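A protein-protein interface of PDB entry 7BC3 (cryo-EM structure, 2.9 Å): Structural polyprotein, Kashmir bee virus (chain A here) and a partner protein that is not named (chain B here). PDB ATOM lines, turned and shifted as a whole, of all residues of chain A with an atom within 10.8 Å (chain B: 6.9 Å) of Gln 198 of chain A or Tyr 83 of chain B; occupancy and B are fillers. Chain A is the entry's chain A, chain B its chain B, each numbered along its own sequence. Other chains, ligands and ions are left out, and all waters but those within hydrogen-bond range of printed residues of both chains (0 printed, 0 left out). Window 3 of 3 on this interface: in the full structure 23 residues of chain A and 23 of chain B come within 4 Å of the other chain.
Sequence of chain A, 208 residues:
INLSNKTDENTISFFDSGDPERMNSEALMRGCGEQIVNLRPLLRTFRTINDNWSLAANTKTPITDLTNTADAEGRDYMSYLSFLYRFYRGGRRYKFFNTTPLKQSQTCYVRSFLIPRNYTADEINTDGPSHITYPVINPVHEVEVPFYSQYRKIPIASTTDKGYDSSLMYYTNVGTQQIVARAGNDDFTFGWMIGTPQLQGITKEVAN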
ATOM      1  N   ALA A  72     -21.939 -32.185 -13.938  1.00  0.00           N
ATOM      2  CA  ALA A  72     -22.188 -31.050 -14.816  1.00  0.00           C
ATOM      3  C   ALA A  72     -22.832 -29.882 -14.085  1.00  0.00           C
ATOM      4  O   ALA A  72     -22.681 -28.735 -14.523  1.00  0.00           O
ATOM      5  CB  ALA A  72     -23.071 -31.467 -15.991  1.00  0.00           C
ATOM      6  N   GLU A  73     -23.539 -30.142 -12.984  1.00  0.00           N
ATOM      7  CA  GLU A  73     -24.208 -29.057 -12.273  1.00  0.00           C
ATOM      8  C   GLU A  73     -23.205 -28.035 -11.748  1.00  0.00           C
ATOM      9  O   GLU A  73     -23.300 -26.841 -12.054  1.00  0.00           O
ATOM     10  CB  GLU A  73     -25.052 -29.622 -11.133  1.00  0.00           C
ATOM     11  CG  GLU A  73     -26.454 -30.013 -11.561  1.00  0.00           C
ATOM     12  CD  GLU A  73     -27.204 -30.776 -10.490  1.00  0.00           C
ATOM     13  OE1 GLU A  73     -26.609 -31.053  -9.427  1.00  0.00           O
ATOM     14  OE2 GLU A  73     -28.388 -31.100 -10.711  1.00  0.00           O
ATOM     15  N   GLY A  74     -22.233 -28.486 -10.958  1.00  0.00           N
ATOM     16  CA  GLY A  74     -21.274 -27.588 -10.346  1.00  0.00           C
ATOM     17  C   GLY A  74     -21.596 -27.183  -8.929  1.00  0.00           C
ATOM     18  O   GLY A  74     -21.092 -26.154  -8.464  1.00  0.00           O
ATOM     19  N   SER A  79     -17.127 -31.137  -8.447  1.00  0.00           N
ATOM     20  CA  SER A  79     -17.639 -30.738  -9.749  1.00  0.00           C
ATOM     21  C   SER A  79     -17.196 -29.328 -10.117  1.00  0.00           C
ATOM     22  O   SER A  79     -16.670 -29.103 -11.210  1.00  0.00           O
ATOM     23  CB  SER A  79     -19.166 -30.825  -9.751  1.00  0.00           C
ATOM     24  OG  SER A  79     -19.689 -30.576 -11.041  1.00  0.00           O
ATOM     25  N   TYR A  80     -17.412 -28.373  -9.211  1.00  0.00           N
ATOM     26  CA  TYR A  80     -16.993 -26.998  -9.448  1.00  0.00           C
ATOM     27  C   TYR A  80     -15.531 -26.933  -9.867  1.00  0.00           C
ATOM     28  O   TYR A  80     -15.177 -26.256 -10.838  1.00  0.00           O
ATOM     29  CB  TYR A  80     -17.224 -26.173  -8.183  1.00  0.00           C
ATOM     30  CG  TYR A  80     -17.252 -24.681  -8.397  1.00  0.00           C
ATOM     31  CD1 TYR A  80     -18.307 -24.074  -9.058  1.00  0.00           C
ATOM     32  CD2 TYR A  80     -16.226 -23.878  -7.928  1.00  0.00           C
ATOM     33  CE1 TYR A  80     -18.334 -22.711  -9.251  1.00  0.00           C
ATOM     34  CE2 TYR A  80     -16.245 -22.517  -8.117  1.00  0.00           C
ATOM     35  CZ  TYR A  80     -17.300 -21.938  -8.776  1.00  0.00           C
ATOM     36  OH  TYR A  80     -17.315 -20.577  -8.959  1.00  0.00           O
ATOM     37  N   PHE A  83     -14.188 -28.303 -13.430  1.00  0.00           N
ATOM     38  CA  PHE A  83     -14.275 -27.411 -14.575  1.00  0.00           C
ATOM     39  C   PHE A  83     -13.019 -26.572 -14.763  1.00  0.00           C
ATOM     40  O   PHE A  83     -12.916 -25.861 -15.768  1.00  0.00           O
ATOM     41  CB  PHE A  83     -15.488 -26.499 -14.420  1.00  0.00           C
ATOM     42  CG  PHE A  83     -16.788 -27.164 -14.755  1.00  0.00           C
ATOM     43  CD1 PHE A  83     -17.236 -27.221 -16.061  1.00  0.00           C
ATOM     44  CD2 PHE A  83     -17.561 -27.737 -13.763  1.00  0.00           C
ATOM     45  CE1 PHE A  83     -18.430 -27.832 -16.368  1.00  0.00           C
ATOM     46  CE2 PHE A  83     -18.755 -28.349 -14.066  1.00  0.00           C
ATOM     47  CZ  PHE A  83     -19.190 -28.397 -15.371  1.00  0.00           C
ATOM     48  N   LEU A  84     -12.074 -26.638 -13.829  1.00  0.00           N
ATOM     49  CA  LEU A  84     -10.792 -25.964 -13.958  1.00  0.00           C
ATOM     50  C   LEU A  84      -9.694 -26.878 -14.469  1.00  0.00           C
ATOM     51  O   LEU A  84      -8.605 -26.392 -14.788  1.00  0.00           O
ATOM     52  CB  LEU A  84     -10.345 -25.403 -12.607  1.00  0.00           C
ATOM     53  CG  LEU A  84     -10.923 -24.086 -12.116  1.00  0.00           C
ATOM     54  CD1 LEU A  84     -10.299 -23.767 -10.781  1.00  0.00           C
ATOM     55  CD2 LEU A  84     -10.668 -22.975 -13.102  1.00  0.00           C
ATOM     56  N   ILE A 194      -6.628 -25.169 -16.370  1.00  0.00           N
ATOM     57  CA  ILE A 194      -7.105 -24.545 -17.589  1.00  0.00           C
ATOM     58  C   ILE A 194      -7.987 -23.364 -17.205  1.00  0.00           C
ATOM     59  O   ILE A 194      -8.149 -23.039 -16.030  1.00  0.00           O
ATOM     60  CB  ILE A 194      -7.877 -25.528 -18.495  1.00  0.00           C
ATOM     61  CG1 ILE A 194      -8.956 -26.250 -17.695  1.00  0.00           C
ATOM     62  CG2 ILE A 194      -6.935 -26.522 -19.145  1.00  0.00           C
ATOM     63  CD1 ILE A 194     -10.127 -26.671 -18.520  1.00  0.00           C
ATOM     64  N   GLY A 195      -8.555 -22.725 -18.214  1.00  0.00           N
ATOM     65  CA  GLY A 195      -9.409 -21.585 -17.984  1.00  0.00           C
ATOM     66  C   GLY A 195     -10.736 -21.969 -17.366  1.00  0.00           C
ATOM     67  O   GLY A 195     -11.101 -23.139 -17.241  1.00  0.00           O
ATOM     68  N   THR A 196     -11.463 -20.948 -16.972  1.00  0.00           N
ATOM     69  CA  THR A 196     -12.731 -21.090 -16.284  1.00  0.00           C
ATOM     70  C   THR A 196     -13.884 -21.126 -17.274  1.00  0.00           C
ATOM     71  O   THR A 196     -13.782 -20.600 -18.385  1.00  0.00           O
ATOM     72  CB  THR A 196     -12.932 -19.926 -15.319  1.00  0.00           C
ATOM     73  OG1 THR A 196     -13.027 -18.705 -16.059  1.00  0.00           O
ATOM     74  CG2 THR A 196     -11.776 -19.827 -14.359  1.00  0.00           C
ATOM     75  N   PRO A 197     -15.003 -21.748 -16.901  1.00  0.00           N
ATOM     76  CA  PRO A 197     -16.232 -21.567 -17.677  1.00  0.00           C
ATOM     77  C   PRO A 197     -17.045 -20.399 -17.153  1.00  0.00           C
ATOM     78  O   PRO A 197     -16.655 -19.754 -16.176  1.00  0.00           O
ATOM     79  CB  PRO A 197     -16.958 -22.899 -17.483  1.00  0.00           C
ATOM     80  CG  PRO A 197     -16.553 -23.333 -16.127  1.00  0.00           C
ATOM     81  CD  PRO A 197     -15.181 -22.758 -15.844  1.00  0.00           C
ATOM     82  N   GLN A 198     -18.174 -20.116 -17.791  1.00  0.00           N
ATOM     83  CA  GLN A 198     -19.050 -19.057 -17.325  1.00  0.00           C
ATOM     84  C   GLN A 198     -19.947 -19.571 -16.208  1.00  0.00           C
ATOM     85  O   GLN A 198     -20.316 -20.748 -16.169  1.00  0.00           O
ATOM     86  CB  GLN A 198     -19.893 -18.520 -18.478  1.00  0.00           C
ATOM     87  CG  GLN A 198     -19.076 -17.821 -19.549  1.00  0.00           C
ATOM     88  CD  GLN A 198     -19.852 -17.592 -20.824  1.00  0.00           C
ATOM     89  OE1 GLN A 198     -19.953 -16.466 -21.309  1.00  0.00           O
ATOM     90  NE2 GLN A 198     -20.403 -18.662 -21.381  1.00  0.00           N
ATOM     91  N   LEU A 199     -20.294 -18.676 -15.289  1.00  0.00           N
ATOM     92  CA  LEU A 199     -21.073 -19.025 -14.113  1.00  0.00           C
ATOM     93  C   LEU A 199     -22.508 -18.534 -14.253  1.00  0.00           C
ATOM     94  O   LEU A 199     -22.775 -17.493 -14.858  1.00  0.00           O
ATOM     95  CB  LEU A 199     -20.453 -18.436 -12.845  1.00  0.00           C
ATOM     96  CG  LEU A 199     -19.068 -18.967 -12.483  1.00  0.00           C
ATOM     97  CD1 LEU A 199     -18.458 -18.162 -11.352  1.00  0.00           C
ATOM     98  CD2 LEU A 199     -19.146 -20.434 -12.109  1.00  0.00           C
ATOM     99  N   GLN A 200     -23.424 -19.305 -13.679  1.00  0.00           N
ATOM    100  CA  GLN A 200     -24.847 -19.002 -13.698  1.00  0.00           C
ATOM    101  C   GLN A 200     -25.240 -18.374 -12.370  1.00  0.00           C
ATOM    102  O   GLN A 200     -24.860 -18.871 -11.306  1.00  0.00           O
ATOM    103  CB  GLN A 200     -25.657 -20.273 -13.950  1.00  0.00           C
ATOM    104  CG  GLN A 200     -27.109 -20.042 -14.300  1.00  0.00           C
ATOM    105  CD  GLN A 200     -27.728 -21.235 -14.998  1.00  0.00           C
ATOM    106  OE1 GLN A 200     -27.025 -22.136 -15.452  1.00  0.00           O
ATOM    107  NE2 GLN A 200     -29.050 -21.251 -15.078  1.00  0.00           N
ATOM    108  N   GLY A 201     -26.002 -17.281 -12.435  1.00  0.00           N
ATOM    109  CA  GLY A 201     -26.425 -16.556 -11.268  1.00  0.00           C
ATOM    110  C   GLY A 201     -27.924 -16.598 -11.061  1.00  0.00           C
ATOM    111  O   GLY A 201     -28.613 -17.554 -11.443  1.00  0.00           O
ATOM    112  N   LEU B  80     -12.045 -11.831 -29.857  1.00  0.00           N
ATOM    113  CA  LEU B  80     -12.567 -12.706 -28.817  1.00  0.00           C
ATOM    114  C   LEU B  80     -13.695 -12.012 -28.063  1.00  0.00           C
ATOM    115  O   LEU B  80     -13.569 -10.850 -27.663  1.00  0.00           O
ATOM    116  CB  LEU B  80     -11.434 -13.090 -27.866  1.00  0.00           C
ATOM    117  CG  LEU B  80     -11.422 -14.464 -27.200  1.00  0.00           C
ATOM    118  CD1 LEU B  80     -11.635 -15.581 -28.194  1.00  0.00           C
ATOM    119  CD2 LEU B  80     -10.095 -14.650 -26.492  1.00  0.00           C
ATOM    120  N   SER B  81     -14.798 -12.726 -27.870  1.00  0.00           N
ATOM    121  CA  SER B  81     -16.003 -12.149 -27.294  1.00  0.00           C
ATOM    122  C   SER B  81     -15.994 -12.255 -25.776  1.00  0.00           C
ATOM    123  O   SER B  81     -15.414 -13.177 -25.198  1.00  0.00           O
ATOM    124  CB  SER B  81     -17.249 -12.838 -27.846  1.00  0.00           C
ATOM    125  OG  SER B  81     -18.417 -12.105 -27.523  1.00  0.00           O
ATOM    126  N   ARG B  82     -16.667 -11.299 -25.135  1.00  0.00           N
ATOM    127  CA  ARG B  82     -16.698 -11.257 -23.677  1.00  0.00           C
ATOM    128  C   ARG B  82     -17.518 -12.408 -23.110  1.00  0.00           C
ATOM    129  O   ARG B  82     -17.113 -13.049 -22.134  1.00  0.00           O
ATOM    130  CB  ARG B  82     -17.258  -9.913 -23.212  1.00  0.00           C
ATOM    131  CG  ARG B  82     -17.332  -9.747 -21.705  1.00  0.00           C
ATOM    132  CD  ARG B  82     -15.955  -9.793 -21.095  1.00  0.00           C
ATOM    133  NE  ARG B  82     -15.962  -9.592 -19.650  1.00  0.00           N
ATOM    134  CZ  ARG B  82     -15.887  -8.407 -19.054  1.00  0.00           C
ATOM    135  NH1 ARG B  82     -15.799  -7.295 -19.768  1.00  0.00           N
ATOM    136  NH2 ARG B  82     -15.897  -8.335 -17.731  1.00  0.00           N
ATOM    137  N   TYR B  83     -18.674 -12.684 -23.707  1.00  0.00           N
ATOM    138  CA  TYR B  83     -19.583 -13.705 -23.217  1.00  0.00           C
ATOM    139  C   TYR B  83     -19.927 -14.686 -24.327  1.00  0.00           C
ATOM    140  O   TYR B  83     -19.797 -14.390 -25.517  1.00  0.00           O
ATOM    141  CB  TYR B  83     -20.872 -13.082 -22.668  1.00  0.00           C
ATOM    142  CG  TYR B  83     -20.646 -12.132 -21.521  1.00  0.00           C
ATOM    143  CD1 TYR B  83     -20.361 -12.606 -20.253  1.00  0.00           C
ATOM    144  CD2 TYR B  83     -20.713 -10.761 -21.708  1.00  0.00           C
ATOM    145  CE1 TYR B  83     -20.152 -11.746 -19.203  1.00  0.00           C
ATOM    146  CE2 TYR B  83     -20.504  -9.890 -20.663  1.00  0.00           C
ATOM    147  CZ  TYR B  83     -20.223 -10.388 -19.412  1.00  0.00           C
ATOM    148  OH  TYR B  83     -20.012  -9.523 -18.365  1.00  0.00           O
ATOM    149  N   VAL B  84     -20.369 -15.871 -23.911  1.00  0.00           N
ATOM    150  CA  VAL B  84     -20.864 -16.886 -24.832  1.00  0.00           C
ATOM    151  C   VAL B  84     -22.141 -17.468 -24.249  1.00  0.00           C
ATOM    152  O   VAL B  84     -22.099 -18.347 -23.381  1.00  0.00           O
ATOM    153  CB  VAL B  84     -19.811 -17.977 -25.085  1.00  0.00           C
ATOM    154  CG1 VAL B  84     -20.384 -19.070 -25.966  1.00  0.00           C
ATOM    155  CG2 VAL B  84     -18.575 -17.368 -25.711  1.00  0.00           C
ATOM    156  N   LEU B  85     -23.281 -16.979 -24.724  1.00  0.00           N
ATOM    157  CA  LEU B  85     -24.574 -17.371 -24.183  1.00  0.00           C
ATOM    158  C   LEU B  85     -25.164 -18.576 -24.892  1.00  0.00           C
ATOM    159  O   LEU B  85     -25.953 -19.315 -24.294  1.00  0.00           O
ATOM    160  CB  LEU B  85     -25.551 -16.198 -24.281  1.00  0.00           C
ATOM    161  CG  LEU B  85     -25.025 -14.856 -23.772  1.00  0.00           C
ATOM    162  CD1 LEU B  85     -26.143 -13.839 -23.714  1.00  0.00           C
ATOM    163  CD2 LEU B  85     -24.375 -15.010 -22.413  1.00  0.00           C
ATOM    164  N   ASP B  86     -24.796 -18.791 -26.150  1.00  0.00           N
ATOM    165  CA  ASP B  86     -25.331 -19.876 -26.952  1.00  0.00           C
ATOM    166  C   ASP B  86     -24.204 -20.525 -27.738  1.00  0.00           C
ATOM    167  O   ASP B  86     -23.195 -19.888 -28.051  1.00  0.00           O
ATOM    168  CB  ASP B  86     -26.409 -19.369 -27.909  1.00  0.00           C
ATOM    169  CG  ASP B  86     -27.613 -18.814 -27.182  1.00  0.00           C
ATOM    170  OD1 ASP B  86     -27.966 -19.354 -26.113  1.00  0.00           O
ATOM    171  OD2 ASP B  86     -28.199 -17.827 -27.673  1.00  0.00           O
ATOM    172  N   ASN B  89     -23.222 -18.963 -31.035  1.00  0.00           N
ATOM    173  CA  ASN B  89     -22.357 -17.786 -31.006  1.00  0.00           C
ATOM    174  C   ASN B  89     -21.057 -18.126 -30.284  1.00  0.00           C
ATOM    175  O   ASN B  89     -20.692 -17.475 -29.297  1.00  0.00           O
ATOM    176  CB  ASN B  89     -23.065 -16.619 -30.325  1.00  0.00           C
ATOM    177  CG  ASN B  89     -24.252 -16.118 -31.117  1.00  0.00           C
ATOM    178  OD1 ASN B  89     -24.195 -16.006 -32.341  1.00  0.00           O
ATOM    179  ND2 ASN B  89     -25.342 -15.821 -30.421  1.00  0.00           N
ATOM    180  N   PRO B  90     -20.334 -19.141 -30.748  1.00  0.00           N
ATOM    181  CA  PRO B  90     -19.102 -19.541 -30.065  1.00  0.00           C
ATOM    182  C   PRO B  90     -17.967 -18.566 -30.332  1.00  0.00           C
ATOM    183  O   PRO B  90     -18.058 -17.655 -31.157  1.00  0.00           O
ATOM    184  CB  PRO B  90     -18.799 -20.914 -30.660  1.00  0.00           C
ATOM    185  CG  PRO B  90     -19.410 -20.884 -32.003  1.00  0.00           C
ATOM    186  CD  PRO B  90     -20.625 -20.008 -31.902  1.00  0.00           C
ATOM    187  N   GLN B  91     -16.875 -18.779 -29.606  1.00  0.00           N
ATOM    188  CA  GLN B  91     -15.661 -18.022 -29.857  1.00  0.00           C
ATOM    189  C   GLN B  91     -15.080 -18.414 -31.207  1.00  0.00           C
ATOM    190  O   GLN B  91     -14.913 -19.599 -31.506  1.00  0.00           O
ATOM    191  CB  GLN B  91     -14.640 -18.271 -28.751  1.00  0.00           C
ATOM    192  CG  GLN B  91     -15.058 -17.748 -27.394  1.00  0.00           C
ATOM    193  CD  GLN B  91     -15.101 -16.236 -27.337  1.00  0.00           C
ATOM    194  OE1 GLN B  91     -14.928 -15.559 -28.349  1.00  0.00           O
ATOM    195  NE2 GLN B  91     -15.333 -15.700 -26.150  1.00  0.00           N
ATOM    196  N   GLU B 153     -19.661 -27.496 -22.372  1.00  0.00           N
ATOM    197  CA  GLU B 153     -19.509 -26.547 -21.277  1.00  0.00           C
ATOM    198  C   GLU B 153     -18.096 -26.524 -20.714  1.00  0.00           C
ATOM    199  O   GLU B 153     -17.779 -25.630 -19.921  1.00  0.00           O
ATOM    200  CB  GLU B 153     -20.507 -26.868 -20.162  1.00  0.00           C
ATOM    201  CG  GLU B 153     -20.385 -28.272 -19.582  1.00  0.00           C
ATOM    202  CD  GLU B 153     -21.287 -29.277 -20.273  1.00  0.00           C
ATOM    203  OE1 GLU B 153     -21.755 -28.989 -21.395  1.00  0.00           O
ATOM    204  OE2 GLU B 153     -21.529 -30.355 -19.692  1.00  0.00           O
ATOM    205  N   TYR B 158     -17.073 -21.994 -26.353  1.00  0.00           N
ATOM    206  CA  TYR B 158     -18.272 -21.970 -25.523  1.00  0.00           C
ATOM    207  C   TYR B 158     -18.008 -21.424 -24.126  1.00  0.00           C
ATOM    208  O   TYR B 158     -18.864 -21.563 -23.245  1.00  0.00           O
ATOM    209  CB  TYR B 158     -18.913 -23.359 -25.406  1.00  0.00           C
ATOM    210  CG  TYR B 158     -19.173 -24.030 -26.733  1.00  0.00           C
ATOM    211  CD1 TYR B 158     -19.586 -23.297 -27.834  1.00  0.00           C
ATOM    212  CD2 TYR B 158     -19.008 -25.397 -26.885  1.00  0.00           C
ATOM    213  CE1 TYR B 158     -19.826 -23.905 -29.048  1.00  0.00           C
ATOM    214  CE2 TYR B 158     -19.246 -26.015 -28.097  1.00  0.00           C
ATOM    215  CZ  TYR B 158     -19.655 -25.263 -29.174  1.00  0.00           C
ATOM    216  OH  TYR B 158     -19.896 -25.863 -30.388  1.00  0.00           O
ATOM    217  N   THR B 159     -16.847 -20.813 -23.893  1.00  0.00           N
ATOM    218  CA  THR B 159     -16.608 -20.082 -22.656  1.00  0.00           C
ATOM    219  C   THR B 159     -16.190 -18.654 -22.978  1.00  0.00           C
ATOM    220  O   THR B 159     -16.251 -18.231 -24.135  1.00  0.00           O
ATOM    221  CB  THR B 159     -15.550 -20.770 -21.787  1.00  0.00           C
ATOM    222  OG1 THR B 159     -15.387 -20.038 -20.567  1.00  0.00           O
ATOM    223  CG2 THR B 159     -14.217 -20.849 -22.494  1.00  0.00           C
ATOM    224  N   SER B 160     -15.757 -17.912 -21.968  1.00  0.00           N
ATOM    225  CA  SER B 160     -15.585 -16.475 -22.099  1.00  0.00           C
ATOM    226  C   SER B 160     -14.146 -16.111 -22.446  1.00  0.00           C
ATOM    227  O   SER B 160     -13.224 -16.924 -22.367  1.00  0.00           O
ATOM    228  CB  SER B 160     -16.000 -15.776 -20.807  1.00  0.00           C
ATOM    229  OG  SER B 160     -15.318 -16.323 -19.693  1.00  0.00           O
ATOM    230  N   ARG B 161     -13.973 -14.849 -22.845  1.00  0.00           N
ATOM    231  CA  ARG B 161     -12.641 -14.309 -23.087  1.00  0.00           C
ATOM    232  C   ARG B 161     -11.733 -14.530 -21.888  1.00  0.00           C
ATOM    233  O   ARG B 161     -10.565 -14.905 -22.041  1.00  0.00           O
ATOM    234  CB  ARG B 161     -12.751 -12.820 -23.406  1.00  0.00           C
ATOM    235  CG  ARG B 161     -11.466 -12.160 -23.827  1.00  0.00           C
ATOM    236  CD  ARG B 161     -11.717 -10.721 -24.205  1.00  0.00           C
ATOM    237  NE  ARG B 161     -12.184  -9.934 -23.070  1.00  0.00           N
ATOM    238  CZ  ARG B 161     -12.870  -8.802 -23.179  1.00  0.00           C
ATOM    239  NH1 ARG B 161     -13.181  -8.316 -24.371  1.00  0.00           N
ATOM    240  NH2 ARG B 161     -13.246  -8.152 -22.090  1.00  0.00           N
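The side-chain hydroxyl of Ser 81 of chain B lies within hydrogen-bond range of the backbone carbonyl oxygen of Tyr 83 of chain B (3.3 Å).
The side-chain amide nitrogen of Gln 91 of chain B lies within hydrogen-bond range of the backbone carbonyl oxygen of Thr 159 of chain B (3.4 Å).
Of the 15 printed residues of chain A, 4 touch a printed residue of chain B.
Hydrophobic or aromatic side chains of chain A within 4 Å of the printed part of chain B: Phe 83 and Pro 197.
Printed residues of chain B that touch a printed residue of chain A: Tyr 83, Val 84, Glu 153, Tyr 158, Thr 159 and Ser 160.
Among the printed residues, 9 pairs touch across the chains.
Phe 83 of chain A touches Glu 153 of chain B.
Pro 197 of chain A touches Glu 153 of chain B (CB to O, 3.8 Å).
Thr 159 of chain B touches Pro 197 of chain A.
Gln 198 of chain A touches Tyr 83 of chain B (OE1 to CA, 3.4 Å).
Tyr 158 of chain B touches Gln 198 of chain A (O to NE2, 3.8 Å).
Gln 198 of chain A touches Thr 159 of chain B (N to OG1, 3.9 Å).
Ser 160 of chain B touches Gln 198 of chain A.
Gln 198 of chain A touches just these residues of chain B: Tyr 83, Val 84, Tyr 158, Thr 159 and Ser 160.
No residue of chain A comes within 4 Å of Ser 81 of chain B.
No residue of chain A comes within 4 Å of Arg 82 of chain B.
Val 84 of chain B touches just one residue of chain A: Gln 198.
No residue of chain A comes within 4 Å of Leu 85 of chain B.
Of chain A, only Gln 198 (3.9 Å) comes within 4 Å of Ser 160 of chain B.
Of the printed residues of chain B, Phe 83 of chain A touches Glu 153 (3.8 Å).
Printed residues of chain B within 4 Å of Thr 196 of chain A: Thr 159.
Of the printed residues of chain A, Tyr 158 of chain B touches Gln 198.
Printed residues of chain A within 4 Å of Glu 153 of chain B: Phe 83 (3.8 Å) and Pro 197 (3.8 Å).
Printed residues of chain B within 4 Å of Pro 197 of chain A: Glu 153 and Thr 159.
Arg 161 of chain B touches none of the printed residues of chain A.
The nearest residue of chain B that does not touch Gln 198 of chain A is Arg 82 of chain B (4.5 Å).
The nearest residue of chain A that does not touch Tyr 83 of chain B is Leu 199 of chain A (7.7 Å).
The nearest printed residue of chain A that does not touch Glu 153 of chain B is Ala 72 of chain A (4.2 Å).
The side-chain amide nitrogen of Gln 198 of chain A sits at hydrogen-bond distance from the backbone carbonyl oxygen of Val 84 of chain B (2.6 Å).
The backbone carbonyl oxygen (O) of Thr 196 of chain A is in hydrogen-bond range of the side-chain hydroxyl (OG1) of Thr 159 of chain B (2.8 Å).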
